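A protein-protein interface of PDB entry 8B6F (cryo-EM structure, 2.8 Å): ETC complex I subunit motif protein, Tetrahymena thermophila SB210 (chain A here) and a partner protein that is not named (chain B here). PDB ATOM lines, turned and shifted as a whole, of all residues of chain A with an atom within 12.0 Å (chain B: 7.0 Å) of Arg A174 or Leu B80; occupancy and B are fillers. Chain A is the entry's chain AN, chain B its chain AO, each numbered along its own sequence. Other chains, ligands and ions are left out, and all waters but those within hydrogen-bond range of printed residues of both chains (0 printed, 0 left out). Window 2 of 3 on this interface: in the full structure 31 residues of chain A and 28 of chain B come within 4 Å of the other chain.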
ATOM      1  N   GLU A 165      21.116  21.025  23.248  1.00  0.00           N
ATOM      2  CA  GLU A 165      22.075  20.111  22.640  1.00  0.00           C
ATOM      3  C   GLU A 165      22.697  19.199  23.689  1.00  0.00           C
ATOM      4  O   GLU A 165      22.847  17.994  23.464  1.00  0.00           O
ATOM      5  CB  GLU A 165      23.153  20.910  21.904  1.00  0.00           C
ATOM      6  CG  GLU A 165      24.422  20.128  21.583  1.00  0.00           C
ATOM      7  CD  GLU A 165      24.152  18.865  20.793  1.00  0.00           C
ATOM      8  OE1 GLU A 165      23.064  18.757  20.189  1.00  0.00           O
ATOM      9  OE2 GLU A 165      25.031  17.977  20.778  1.00  0.00           O
ATOM     10  N   MET A 166      23.069  19.759  24.841  1.00  0.00           N
ATOM     11  CA  MET A 166      23.634  18.941  25.910  1.00  0.00           C
ATOM     12  C   MET A 166      22.635  17.888  26.378  1.00  0.00           C
ATOM     13  O   MET A 166      22.997  16.724  26.583  1.00  0.00           O
ATOM     14  CB  MET A 166      24.066  19.838  27.071  1.00  0.00           C
ATOM     15  CG  MET A 166      24.887  19.134  28.147  1.00  0.00           C
ATOM     16  SD  MET A 166      23.922  18.118  29.285  1.00  0.00           S
ATOM     17  CE  MET A 166      22.892  19.350  30.076  1.00  0.00           C
ATOM     18  N   ILE A 167      21.375  18.285  26.571  1.00  0.00           N
ATOM     19  CA  ILE A 167      20.354  17.339  27.015  1.00  0.00           C
ATOM     20  C   ILE A 167      20.159  16.239  25.980  1.00  0.00           C
ATOM     21  O   ILE A 167      20.043  15.056  26.323  1.00  0.00           O
ATOM     22  CB  ILE A 167      19.033  18.076  27.311  1.00  0.00           C
ATOM     23  CG1 ILE A 167      19.196  19.027  28.504  1.00  0.00           C
ATOM     24  CG2 ILE A 167      17.900  17.080  27.565  1.00  0.00           C
ATOM     25  CD1 ILE A 167      19.526  18.349  29.822  1.00  0.00           C
ATOM     26  N   ARG A 168      20.115  16.607  24.699  1.00  0.00           N
ATOM     27  CA  ARG A 168      19.924  15.612  23.649  1.00  0.00           C
ATOM     28  C   ARG A 168      21.063  14.601  23.631  1.00  0.00           C
ATOM     29  O   ARG A 168      20.832  13.389  23.565  1.00  0.00           O
ATOM     30  CB  ARG A 168      19.804  16.305  22.290  1.00  0.00           C
ATOM     31  CG  ARG A 168      19.505  15.355  21.135  1.00  0.00           C
ATOM     32  CD  ARG A 168      19.752  16.015  19.789  1.00  0.00           C
ATOM     33  NE  ARG A 168      21.157  16.362  19.600  1.00  0.00           N
ATOM     34  CZ  ARG A 168      22.098  15.508  19.224  1.00  0.00           C
ATOM     35  NH1 ARG A 168      21.825  14.232  18.999  1.00  0.00           N
ATOM     36  NH2 ARG A 168      23.344  15.942  19.067  1.00  0.00           N
ATOM     37  N   ILE A 169      22.306  15.081  23.691  1.00  0.00           N
ATOM     38  CA  ILE A 169      23.437  14.164  23.614  1.00  0.00           C
ATOM     39  C   ILE A 169      23.512  13.288  24.857  1.00  0.00           C
ATOM     40  O   ILE A 169      24.000  12.153  24.794  1.00  0.00           O
ATOM     41  CB  ILE A 169      24.746  14.946  23.389  1.00  0.00           C
ATOM     42  CG1 ILE A 169      25.917  13.991  23.148  1.00  0.00           C
ATOM     43  CG2 ILE A 169      25.052  15.848  24.571  1.00  0.00           C
ATOM     44  CD1 ILE A 169      25.741  13.099  21.940  1.00  0.00           C
ATOM     45  N   ALA A 170      23.044  13.788  26.002  1.00  0.00           N
ATOM     46  CA  ALA A 170      23.074  12.999  27.225  1.00  0.00           C
ATOM     47  C   ALA A 170      22.132  11.803  27.187  1.00  0.00           C
ATOM     48  O   ALA A 170      22.234  10.935  28.060  1.00  0.00           O
ATOM     49  CB  ALA A 170      22.722  13.883  28.423  1.00  0.00           C
ATOM     50  N   SER A 171      21.219  11.737  26.220  1.00  0.00           N
ATOM     51  CA  SER A 171      20.203  10.694  26.174  1.00  0.00           C
ATOM     52  C   SER A 171      20.508   9.610  25.149  1.00  0.00           C
ATOM     53  O   SER A 171      19.661   8.743  24.914  1.00  0.00           O
ATOM     54  CB  SER A 171      18.833  11.309  25.882  1.00  0.00           C
ATOM     55  OG  SER A 171      18.816  11.928  24.607  1.00  0.00           O
ATOM     56  N   GLN A 172      21.687   9.634  24.534  1.00  0.00           N
ATOM     57  CA  GLN A 172      22.017   8.661  23.505  1.00  0.00           C
ATOM     58  C   GLN A 172      22.366   7.311  24.121  1.00  0.00           C
ATOM     59  O   GLN A 172      22.883   7.228  25.238  1.00  0.00           O
ATOM     60  CB  GLN A 172      23.189   9.157  22.655  1.00  0.00           C
ATOM     61  CG  GLN A 172      22.939  10.484  21.959  1.00  0.00           C
ATOM     62  CD  GLN A 172      21.790  10.422  20.973  1.00  0.00           C
ATOM     63  OE1 GLN A 172      21.379   9.344  20.547  1.00  0.00           O
ATOM     64  NE2 GLN A 172      21.262  11.585  20.605  1.00  0.00           N
ATOM     65  N   LYS A 173      22.067   6.247  23.379  1.00  0.00           N
ATOM     66  CA  LYS A 173      22.470   4.909  23.786  1.00  0.00           C
ATOM     67  C   LYS A 173      23.986   4.764  23.691  1.00  0.00           C
ATOM     68  O   LYS A 173      24.630   5.327  22.803  1.00  0.00           O
ATOM     69  CB  LYS A 173      21.787   3.857  22.911  1.00  0.00           C
ATOM     70  CG  LYS A 173      22.184   2.421  23.237  1.00  0.00           C
ATOM     71  CD  LYS A 173      21.580   1.439  22.250  1.00  0.00           C
ATOM     72  CE  LYS A 173      22.127   0.036  22.470  1.00  0.00           C
ATOM     73  NZ  LYS A 173      21.631  -0.928  21.447  1.00  0.00           N
ATOM     74  N   ARG A 174      24.557   3.997  24.619  1.00  0.00           N
ATOM     75  CA  ARG A 174      25.999   3.815  24.687  1.00  0.00           C
ATOM     76  C   ARG A 174      26.336   2.333  24.759  1.00  0.00           C
ATOM     77  O   ARG A 174      25.666   1.568  25.459  1.00  0.00           O
ATOM     78  CB  ARG A 174      26.587   4.548  25.897  1.00  0.00           C
ATOM     79  CG  ARG A 174      26.065   4.055  27.236  1.00  0.00           C
ATOM     80  CD  ARG A 174      26.449   4.997  28.368  1.00  0.00           C
ATOM     81  NE  ARG A 174      25.706   6.252  28.317  1.00  0.00           N
ATOM     82  CZ  ARG A 174      26.126   7.360  27.717  1.00  0.00           C
ATOM     83  NH1 ARG A 174      27.293   7.415  27.097  1.00  0.00           N
ATOM     84  NH2 ARG A 174      25.353   8.442  27.742  1.00  0.00           N
ATOM     85  N   VAL A 175      27.379   1.939  24.028  1.00  0.00           N
ATOM     86  CA  VAL A 175      27.868   0.567  24.011  1.00  0.00           C
ATOM     87  C   VAL A 175      29.383   0.599  24.164  1.00  0.00           C
ATOM     88  O   VAL A 175      30.024   1.640  24.007  1.00  0.00           O
ATOM     89  CB  VAL A 175      27.465  -0.183  22.725  1.00  0.00           C
ATOM     90  CG1 VAL A 175      25.952  -0.257  22.612  1.00  0.00           C
ATOM     91  CG2 VAL A 175      28.062   0.488  21.497  1.00  0.00           C
ATOM     92  N   TYR A 176      29.951  -0.562  24.480  1.00  0.00           N
ATOM     93  CA  TYR A 176      31.370  -0.688  24.784  1.00  0.00           C
ATOM     94  C   TYR A 176      32.070  -1.558  23.750  1.00  0.00           C
ATOM     95  O   TYR A 176      31.513  -2.554  23.280  1.00  0.00           O
ATOM     96  CB  TYR A 176      31.572  -1.273  26.186  1.00  0.00           C
ATOM     97  CG  TYR A 176      31.008  -0.400  27.283  1.00  0.00           C
ATOM     98  CD1 TYR A 176      29.671  -0.489  27.651  1.00  0.00           C
ATOM     99  CD2 TYR A 176      31.807   0.521  27.942  1.00  0.00           C
ATOM    100  CE1 TYR A 176      29.150   0.311  28.650  1.00  0.00           C
ATOM    101  CE2 TYR A 176      31.296   1.327  28.941  1.00  0.00           C
ATOM    102  CZ  TYR A 176      29.969   1.217  29.290  1.00  0.00           C
ATOM    103  OH  TYR A 176      29.459   2.018  30.284  1.00  0.00           O
ATOM    104  N   LEU A 177      33.299  -1.169  23.395  1.00  0.00           N
ATOM    105  CA  LEU A 177      34.080  -1.936  22.428  1.00  0.00           C
ATOM    106  C   LEU A 177      34.321  -3.360  22.901  1.00  0.00           C
ATOM    107  O   LEU A 177      34.426  -4.277  22.079  1.00  0.00           O
ATOM    108  CB  LEU A 177      35.420  -1.244  22.171  1.00  0.00           C
ATOM    109  CG  LEU A 177      35.404   0.063  21.384  1.00  0.00           C
ATOM    110  CD1 LEU A 177      36.671   0.847  21.618  1.00  0.00           C
ATOM    111  CD2 LEU A 177      35.315  -0.274  19.905  1.00  0.00           C
ATOM    112  N   LYS A 178      34.420  -3.568  24.214  1.00  0.00           N
ATOM    113  CA  LYS A 178      34.755  -4.893  24.720  1.00  0.00           C
ATOM    114  C   LYS A 178      33.705  -5.918  24.316  1.00  0.00           C
ATOM    115  O   LYS A 178      34.035  -7.071  24.018  1.00  0.00           O
ATOM    116  CB  LYS A 178      34.907  -4.847  26.240  1.00  0.00           C
ATOM    117  CG  LYS A 178      35.401  -6.146  26.849  1.00  0.00           C
ATOM    118  CD  LYS A 178      35.554  -6.029  28.358  1.00  0.00           C
ATOM    119  CE  LYS A 178      36.110  -7.314  28.951  1.00  0.00           C
ATOM    120  NZ  LYS A 178      36.249  -7.233  30.431  1.00  0.00           N
ATOM    121  N   HIS A 179      32.436  -5.519  24.299  1.00  0.00           N
ATOM    122  CA  HIS A 179      31.339  -6.430  24.007  1.00  0.00           C
ATOM    123  C   HIS A 179      30.931  -6.433  22.540  1.00  0.00           C
ATOM    124  O   HIS A 179      29.976  -7.130  22.184  1.00  0.00           O
ATOM    125  CB  HIS A 179      30.126  -6.075  24.866  1.00  0.00           C
ATOM    126  CG  HIS A 179      30.399  -6.124  26.336  1.00  0.00           C
ATOM    127  ND1 HIS A 179      30.716  -7.292  26.996  1.00  0.00           N
ATOM    128  CD2 HIS A 179      30.397  -5.149  27.274  1.00  0.00           C
ATOM    129  CE1 HIS A 179      30.904  -7.033  28.277  1.00  0.00           C
ATOM    130  NE2 HIS A 179      30.715  -5.740  28.472  1.00  0.00           N
ATOM    131  N   GLN A 180      31.618  -5.683  21.685  1.00  0.00           N
ATOM    132  CA  GLN A 180      31.298  -5.677  20.265  1.00  0.00           C
ATOM    133  C   GLN A 180      31.964  -6.859  19.575  1.00  0.00           C
ATOM    134  O   GLN A 180      33.168  -7.087  19.734  1.00  0.00           O
ATOM    135  CB  GLN A 180      31.739  -4.366  19.616  1.00  0.00           C
ATOM    136  CG  GLN A 180      30.788  -3.211  19.870  1.00  0.00           C
ATOM    137  CD  GLN A 180      31.092  -2.011  18.996  1.00  0.00           C
ATOM    138  OE1 GLN A 180      32.211  -1.851  18.510  1.00  0.00           O
ATOM    139  NE2 GLN A 180      30.091  -1.164  18.786  1.00  0.00           N
ATOM    140  N   LEU B  73      31.565   4.246  34.628  1.00  0.00           N
ATOM    141  CA  LEU B  73      30.888   3.207  35.397  1.00  0.00           C
ATOM    142  C   LEU B  73      31.813   2.002  35.496  1.00  0.00           C
ATOM    143  O   LEU B  73      32.066   1.319  34.499  1.00  0.00           O
ATOM    144  CB  LEU B  73      29.562   2.829  34.744  1.00  0.00           C
ATOM    145  CG  LEU B  73      28.474   3.902  34.760  1.00  0.00           C
ATOM    146  CD1 LEU B  73      27.259   3.429  33.991  1.00  0.00           C
ATOM    147  CD2 LEU B  73      28.089   4.270  36.183  1.00  0.00           C
ATOM    148  N   ASN B  76      28.626  -2.924  36.726  1.00  0.00           N
ATOM    149  CA  ASN B  76      27.238  -2.918  36.271  1.00  0.00           C
ATOM    150  C   ASN B  76      27.025  -1.863  35.189  1.00  0.00           C
ATOM    151  O   ASN B  76      26.112  -1.039  35.255  1.00  0.00           O
ATOM    152  CB  ASN B  76      26.285  -2.694  37.444  1.00  0.00           C
ATOM    153  CG  ASN B  76      26.339  -3.814  38.460  1.00  0.00           C
ATOM    154  OD1 ASN B  76      26.584  -4.968  38.113  1.00  0.00           O
ATOM    155  ND2 ASN B  76      26.113  -3.478  39.723  1.00  0.00           N
ATOM    156  N   GLN B  77      27.894  -1.894  34.177  1.00  0.00           N
ATOM    157  CA  GLN B  77      27.809  -0.909  33.105  1.00  0.00           C
ATOM    158  C   GLN B  77      26.512  -1.056  32.320  1.00  0.00           C
ATOM    159  O   GLN B  77      25.889  -0.057  31.942  1.00  0.00           O
ATOM    160  CB  GLN B  77      29.013  -1.034  32.171  1.00  0.00           C
ATOM    161  CG  GLN B  77      30.337  -0.616  32.790  1.00  0.00           C
ATOM    162  CD  GLN B  77      30.908  -1.660  33.727  1.00  0.00           C
ATOM    163  OE1 GLN B  77      30.237  -2.630  34.077  1.00  0.00           O
ATOM    164  NE2 GLN B  77      32.157  -1.471  34.132  1.00  0.00           N
ATOM    165  N   ASN B  78      26.088  -2.294  32.066  1.00  0.00           N
ATOM    166  CA  ASN B  78      24.901  -2.522  31.251  1.00  0.00           C
ATOM    167  C   ASN B  78      23.615  -2.120  31.961  1.00  0.00           C
ATOM    168  O   ASN B  78      22.617  -1.840  31.290  1.00  0.00           O
ATOM    169  CB  ASN B  78      24.827  -3.993  30.842  1.00  0.00           C
ATOM    170  CG  ASN B  78      23.635  -4.291  29.958  1.00  0.00           C
ATOM    171  OD1 ASN B  78      22.587  -4.725  30.434  1.00  0.00           O
ATOM    172  ND2 ASN B  78      23.788  -4.055  28.661  1.00  0.00           N
ATOM    173  N   ASP B  79      23.613  -2.085  33.293  1.00  0.00           N
ATOM    174  CA  ASP B  79      22.402  -1.756  34.035  1.00  0.00           C
ATOM    175  C   ASP B  79      22.010  -0.290  33.919  1.00  0.00           C
ATOM    176  O   ASP B  79      20.887   0.061  34.293  1.00  0.00           O
ATOM    177  CB  ASP B  79      22.578  -2.117  35.511  1.00  0.00           C
ATOM    178  CG  ASP B  79      22.803  -3.599  35.724  1.00  0.00           C
ATOM    179  OD1 ASP B  79      22.427  -4.390  34.834  1.00  0.00           O
ATOM    180  OD2 ASP B  79      23.350  -3.974  36.781  1.00  0.00           O
ATOM    181  N   LEU B  80      22.894   0.568  33.415  1.00  0.00           N
ATOM    182  CA  LEU B  80      22.569   1.980  33.288  1.00  0.00           C
ATOM    183  C   LEU B  80      21.350   2.167  32.395  1.00  0.00           C
ATOM    184  O   LEU B  80      21.217   1.523  31.352  1.00  0.00           O
ATOM    185  CB  LEU B  80      23.761   2.748  32.713  1.00  0.00           C
ATOM    186  CG  LEU B  80      23.602   4.269  32.638  1.00  0.00           C
ATOM    187  CD1 LEU B  80      23.593   4.879  34.031  1.00  0.00           C
ATOM    188  CD2 LEU B  80      24.691   4.891  31.781  1.00  0.00           C
ATOM    189  N   ASP B  81      20.456   3.059  32.814  1.00  0.00           N
ATOM    190  CA  ASP B  81      19.253   3.388  32.066  1.00  0.00           C
ATOM    191  C   ASP B  81      19.275   4.861  31.689  1.00  0.00           C
ATOM    192  O   ASP B  81      19.915   5.681  32.355  1.00  0.00           O
ATOM    193  CB  ASP B  81      17.990   3.069  32.875  1.00  0.00           C
ATOM    194  CG  ASP B  81      18.017   3.680  34.259  1.00  0.00           C
ATOM    195  OD1 ASP B  81      19.003   4.375  34.579  1.00  0.00           O
ATOM    196  OD2 ASP B  81      17.058   3.463  35.028  1.00  0.00           O
ATOM    197  N   LYS B  82      18.563   5.196  30.611  1.00  0.00           N
ATOM    198  CA  LYS B  82      18.612   6.553  30.081  1.00  0.00           C
ATOM    199  C   LYS B  82      18.037   7.580  31.049  1.00  0.00           C
ATOM    200  O   LYS B  82      18.289   8.777  30.880  1.00  0.00           O
ATOM    201  CB  LYS B  82      17.869   6.617  28.747  1.00  0.00           C
ATOM    202  CG  LYS B  82      18.483   5.735  27.670  1.00  0.00           C
ATOM    203  CD  LYS B  82      17.800   5.922  26.324  1.00  0.00           C
ATOM    204  CE  LYS B  82      18.459   5.063  25.253  1.00  0.00           C
ATOM    205  NZ  LYS B  82      17.847   5.269  23.910  1.00  0.00           N
ATOM    206  N   THR B  83      17.272   7.147  32.049  1.00  0.00           N
ATOM    207  CA  THR B  83      16.710   8.060  33.035  1.00  0.00           C
ATOM    208  C   THR B  83      17.662   8.358  34.187  1.00  0.00           C
ATOM    209  O   THR B  83      17.385   9.267  34.975  1.00  0.00           O
ATOM    210  CB  THR B  83      15.401   7.496  33.600  1.00  0.00           C
ATOM    211  OG1 THR B  83      15.654   6.245  34.253  1.00  0.00           O
ATOM    212  CG2 THR B  83      14.382   7.290  32.487  1.00  0.00           C
ATOM    213  N   ASN B  84      18.765   7.625  34.305  1.00  0.00           N
ATOM    214  CA  ASN B  84      19.695   7.847  35.401  1.00  0.00           C
ATOM    215  C   ASN B  84      20.422   9.177  35.239  1.00  0.00           C
ATOM    216  O   ASN B  84      20.666   9.648  34.125  1.00  0.00           O
ATOM    217  CB  ASN B  84      20.713   6.710  35.481  1.00  0.00           C
ATOM    218  CG  ASN B  84      20.427   5.749  36.617  1.00  0.00           C
ATOM    219  OD1 ASN B  84      19.990   6.154  37.694  1.00  0.00           O
ATOM    220  ND2 ASN B  84      20.673   4.465  36.381  1.00  0.00           N
ATOM    221  N   ILE B  85      20.771   9.784  36.376  1.00  0.00           N
ATOM    222  CA  ILE B  85      21.469  11.062  36.356  1.00  0.00           C
ATOM    223  C   ILE B  85      22.905  10.915  35.877  1.00  0.00           C
ATOM    224  O   ILE B  85      23.508  11.897  35.431  1.00  0.00           O
ATOM    225  CB  ILE B  85      21.425  11.710  37.753  1.00  0.00           C
ATOM    226  CG1 ILE B  85      21.942  13.150  37.683  1.00  0.00           C
ATOM    227  CG2 ILE B  85      22.237  10.888  38.750  1.00  0.00           C
ATOM    228  CD1 ILE B  85      21.817  13.918  38.983  1.00  0.00           C
ATOM    229  N   GLU B  86      23.475   9.711  35.950  1.00  0.00           N
ATOM    230  CA  GLU B  86      24.860   9.519  35.538  1.00  0.00           C
ATOM    231  C   GLU B  86      25.059   9.772  34.052  1.00  0.00           C
ATOM    232  O   GLU B  86      26.185  10.056  33.630  1.00  0.00           O
ATOM    233  CB  GLU B  86      25.328   8.103  35.883  1.00  0.00           C
ATOM    234  CG  GLU B  86      25.504   7.847  37.373  1.00  0.00           C
ATOM    235  CD  GLU B  86      24.185   7.683  38.107  1.00  0.00           C
ATOM    236  OE1 GLU B  86      23.205   7.230  37.480  1.00  0.00           O
ATOM    237  OE2 GLU B  86      24.129   8.009  39.310  1.00  0.00           O
ATOM    238  N   ASN B  87      23.999   9.676  33.248  1.00  0.00           N
ATOM    239  CA  ASN B  87      24.142   9.874  31.811  1.00  0.00           C
ATOM    240  C   ASN B  87      24.617  11.276  31.467  1.00  0.00           C
ATOM    241  O   ASN B  87      25.208  11.474  30.400  1.00  0.00           O
ATOM    242  CB  ASN B  87      22.812   9.596  31.113  1.00  0.00           C
ATOM    243  CG  ASN B  87      22.321   8.185  31.345  1.00  0.00           C
ATOM    244  OD1 ASN B  87      22.669   7.263  30.610  1.00  0.00           O
ATOM    245  ND2 ASN B  87      21.503   8.008  32.376  1.00  0.00           N
ATOM    246  N   TYR B  88      24.371  12.254  32.339  1.00  0.00           N
ATOM    247  CA  TYR B  88      24.800  13.621  32.086  1.00  0.00           C
ATOM    248  C   TYR B  88      26.250  13.872  32.476  1.00  0.00           C
ATOM    249  O   TYR B  88      26.781  14.939  32.156  1.00  0.00           O
ATOM    250  CB  TYR B  88      23.888  14.597  32.833  1.00  0.00           C
ATOM    251  CG  TYR B  88      22.433  14.466  32.447  1.00  0.00           C
ATOM    252  CD1 TYR B  88      21.917  15.162  31.362  1.00  0.00           C
ATOM    253  CD2 TYR B  88      21.578  13.639  33.161  1.00  0.00           C
ATOM    254  CE1 TYR B  88      20.589  15.042  31.001  1.00  0.00           C
ATOM    255  CE2 TYR B  88      20.249  13.512  32.810  1.00  0.00           C
ATOM    256  CZ  TYR B  88      19.760  14.216  31.729  1.00  0.00           C
ATOM    257  OH  TYR B  88      18.437  14.092  31.375  1.00  0.00           O
ATOM    258  N   PHE B  90      28.925  11.949  31.475  1.00  0.00           N
ATOM    259  CA  PHE B  90      29.836  11.599  30.394  1.00  0.00           C
ATOM    260  C   PHE B  90      30.017  12.766  29.432  1.00  0.00           C
ATOM    261  O   PHE B  90      29.046  13.401  29.013  1.00  0.00           O
ATOM    262  CB  PHE B  90      29.313  10.375  29.643  1.00  0.00           C
ATOM    263  CG  PHE B  90      29.041   9.192  30.526  1.00  0.00           C
ATOM    264  CD1 PHE B  90      30.084   8.426  31.019  1.00  0.00           C
ATOM    265  CD2 PHE B  90      27.744   8.836  30.853  1.00  0.00           C
ATOM    266  CE1 PHE B  90      29.839   7.334  31.828  1.00  0.00           C
ATOM    267  CE2 PHE B  90      27.492   7.745  31.661  1.00  0.00           C
ATOM    268  CZ  PHE B  90      28.541   6.993  32.149  1.00  0.00           C
ATOM    269  N   LYS B  91      31.273  13.041  29.080  1.00  0.00           N
ATOM    270  CA  LYS B  91      31.664  14.001  28.051  1.00  0.00           C
ATOM    271  C   LYS B  91      31.436  15.452  28.455  1.00  0.00           C
ATOM    272  O   LYS B  91      31.641  16.351  27.630  1.00  0.00           O
ATOM    273  CB  LYS B  91      30.938  13.727  26.729  1.00  0.00           C
ATOM    274  CG  LYS B  91      31.094  12.296  26.237  1.00  0.00           C
ATOM    275  CD  LYS B  91      30.397  12.074  24.905  1.00  0.00           C
ATOM    276  CE  LYS B  91      31.118  12.769  23.759  1.00  0.00           C
ATOM    277  NZ  LYS B  91      32.516  12.283  23.585  1.00  0.00           N
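Among the printed residues, merely in contact across the chains: Ala A170 with Tyr B88 (3.3 Å), Ala A170 with Asn B87 (3.4 Å), Tyr A176 with Gln B77 (3.6 Å), Ser A171 with Lys B82 (3.7 Å), Ile A167 with Tyr B88 (3.7 Å), Arg A174 with Phe B90 (3.8 Å), Arg A174 with Leu B80 (3.8 Å) and Arg A174 with Asn B87 (3.9 Å).
Of chain B, only Leu B80 (3.8 Å), Asn B87 (3.9 Å) and Phe B90 (3.8 Å) come within 4 Å of Arg A174.
Of chain A, only Arg A174 (3.8 Å) comes within 4 Å of Leu B80.
No residue of chain A comes within 4 Å of Asn B78.
No residue of chain A comes within 4 Å of Asn B84.
Glu B86 touches none of the printed residues of chain A.
Of chain A, only Ala A170 (3.4 Å) and Arg A174 (3.9 Å) come within 4 Å of Asn B87.
Phe B90 touches one residue of chain A.
Of the printed residues of chain A, Gln B77 touches Tyr A176 (3.6 Å).
Of the printed residues of chain A, Tyr B88 touches Ile A167 and Ala A170.
Of the printed residues of chain B, Ser A171 touches Lys B82 (3.7 Å).
Thr B83 touches none of the printed residues of chain A.
Lys B91 touches none of the printed residues of chain A.
The nearest residue of chain A that does not touch Leu B80 is Tyr A176 (5.8 Å).
The backbone carbonyl oxygen (O) of Arg A168 sits at hydrogen-bond distance from the side-chain hydroxyl (OG) of Ser A171, 2.7 Å away.
The side-chain amide nitrogen (NE2) of Gln B77 lies within hydrogen-bond range of the backbone carbonyl oxygen (O) of Leu B73 (2.8 Å).
The backbone carbonyl oxygen (O) of Asp B81 lies within hydrogen-bond range of the side-chain amide nitrogen (ND2) of Asn B87 (2.8 Å).
ND2 of Asn B87 is in hydrogen-bond range of O of Asn B84, 2.5 Å away.
Along chain B the printed residues that touch a printed residue of chain A span positions 77 to 90.
Of the 16 printed residues of chain A, 5 touch a printed residue of chain B.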
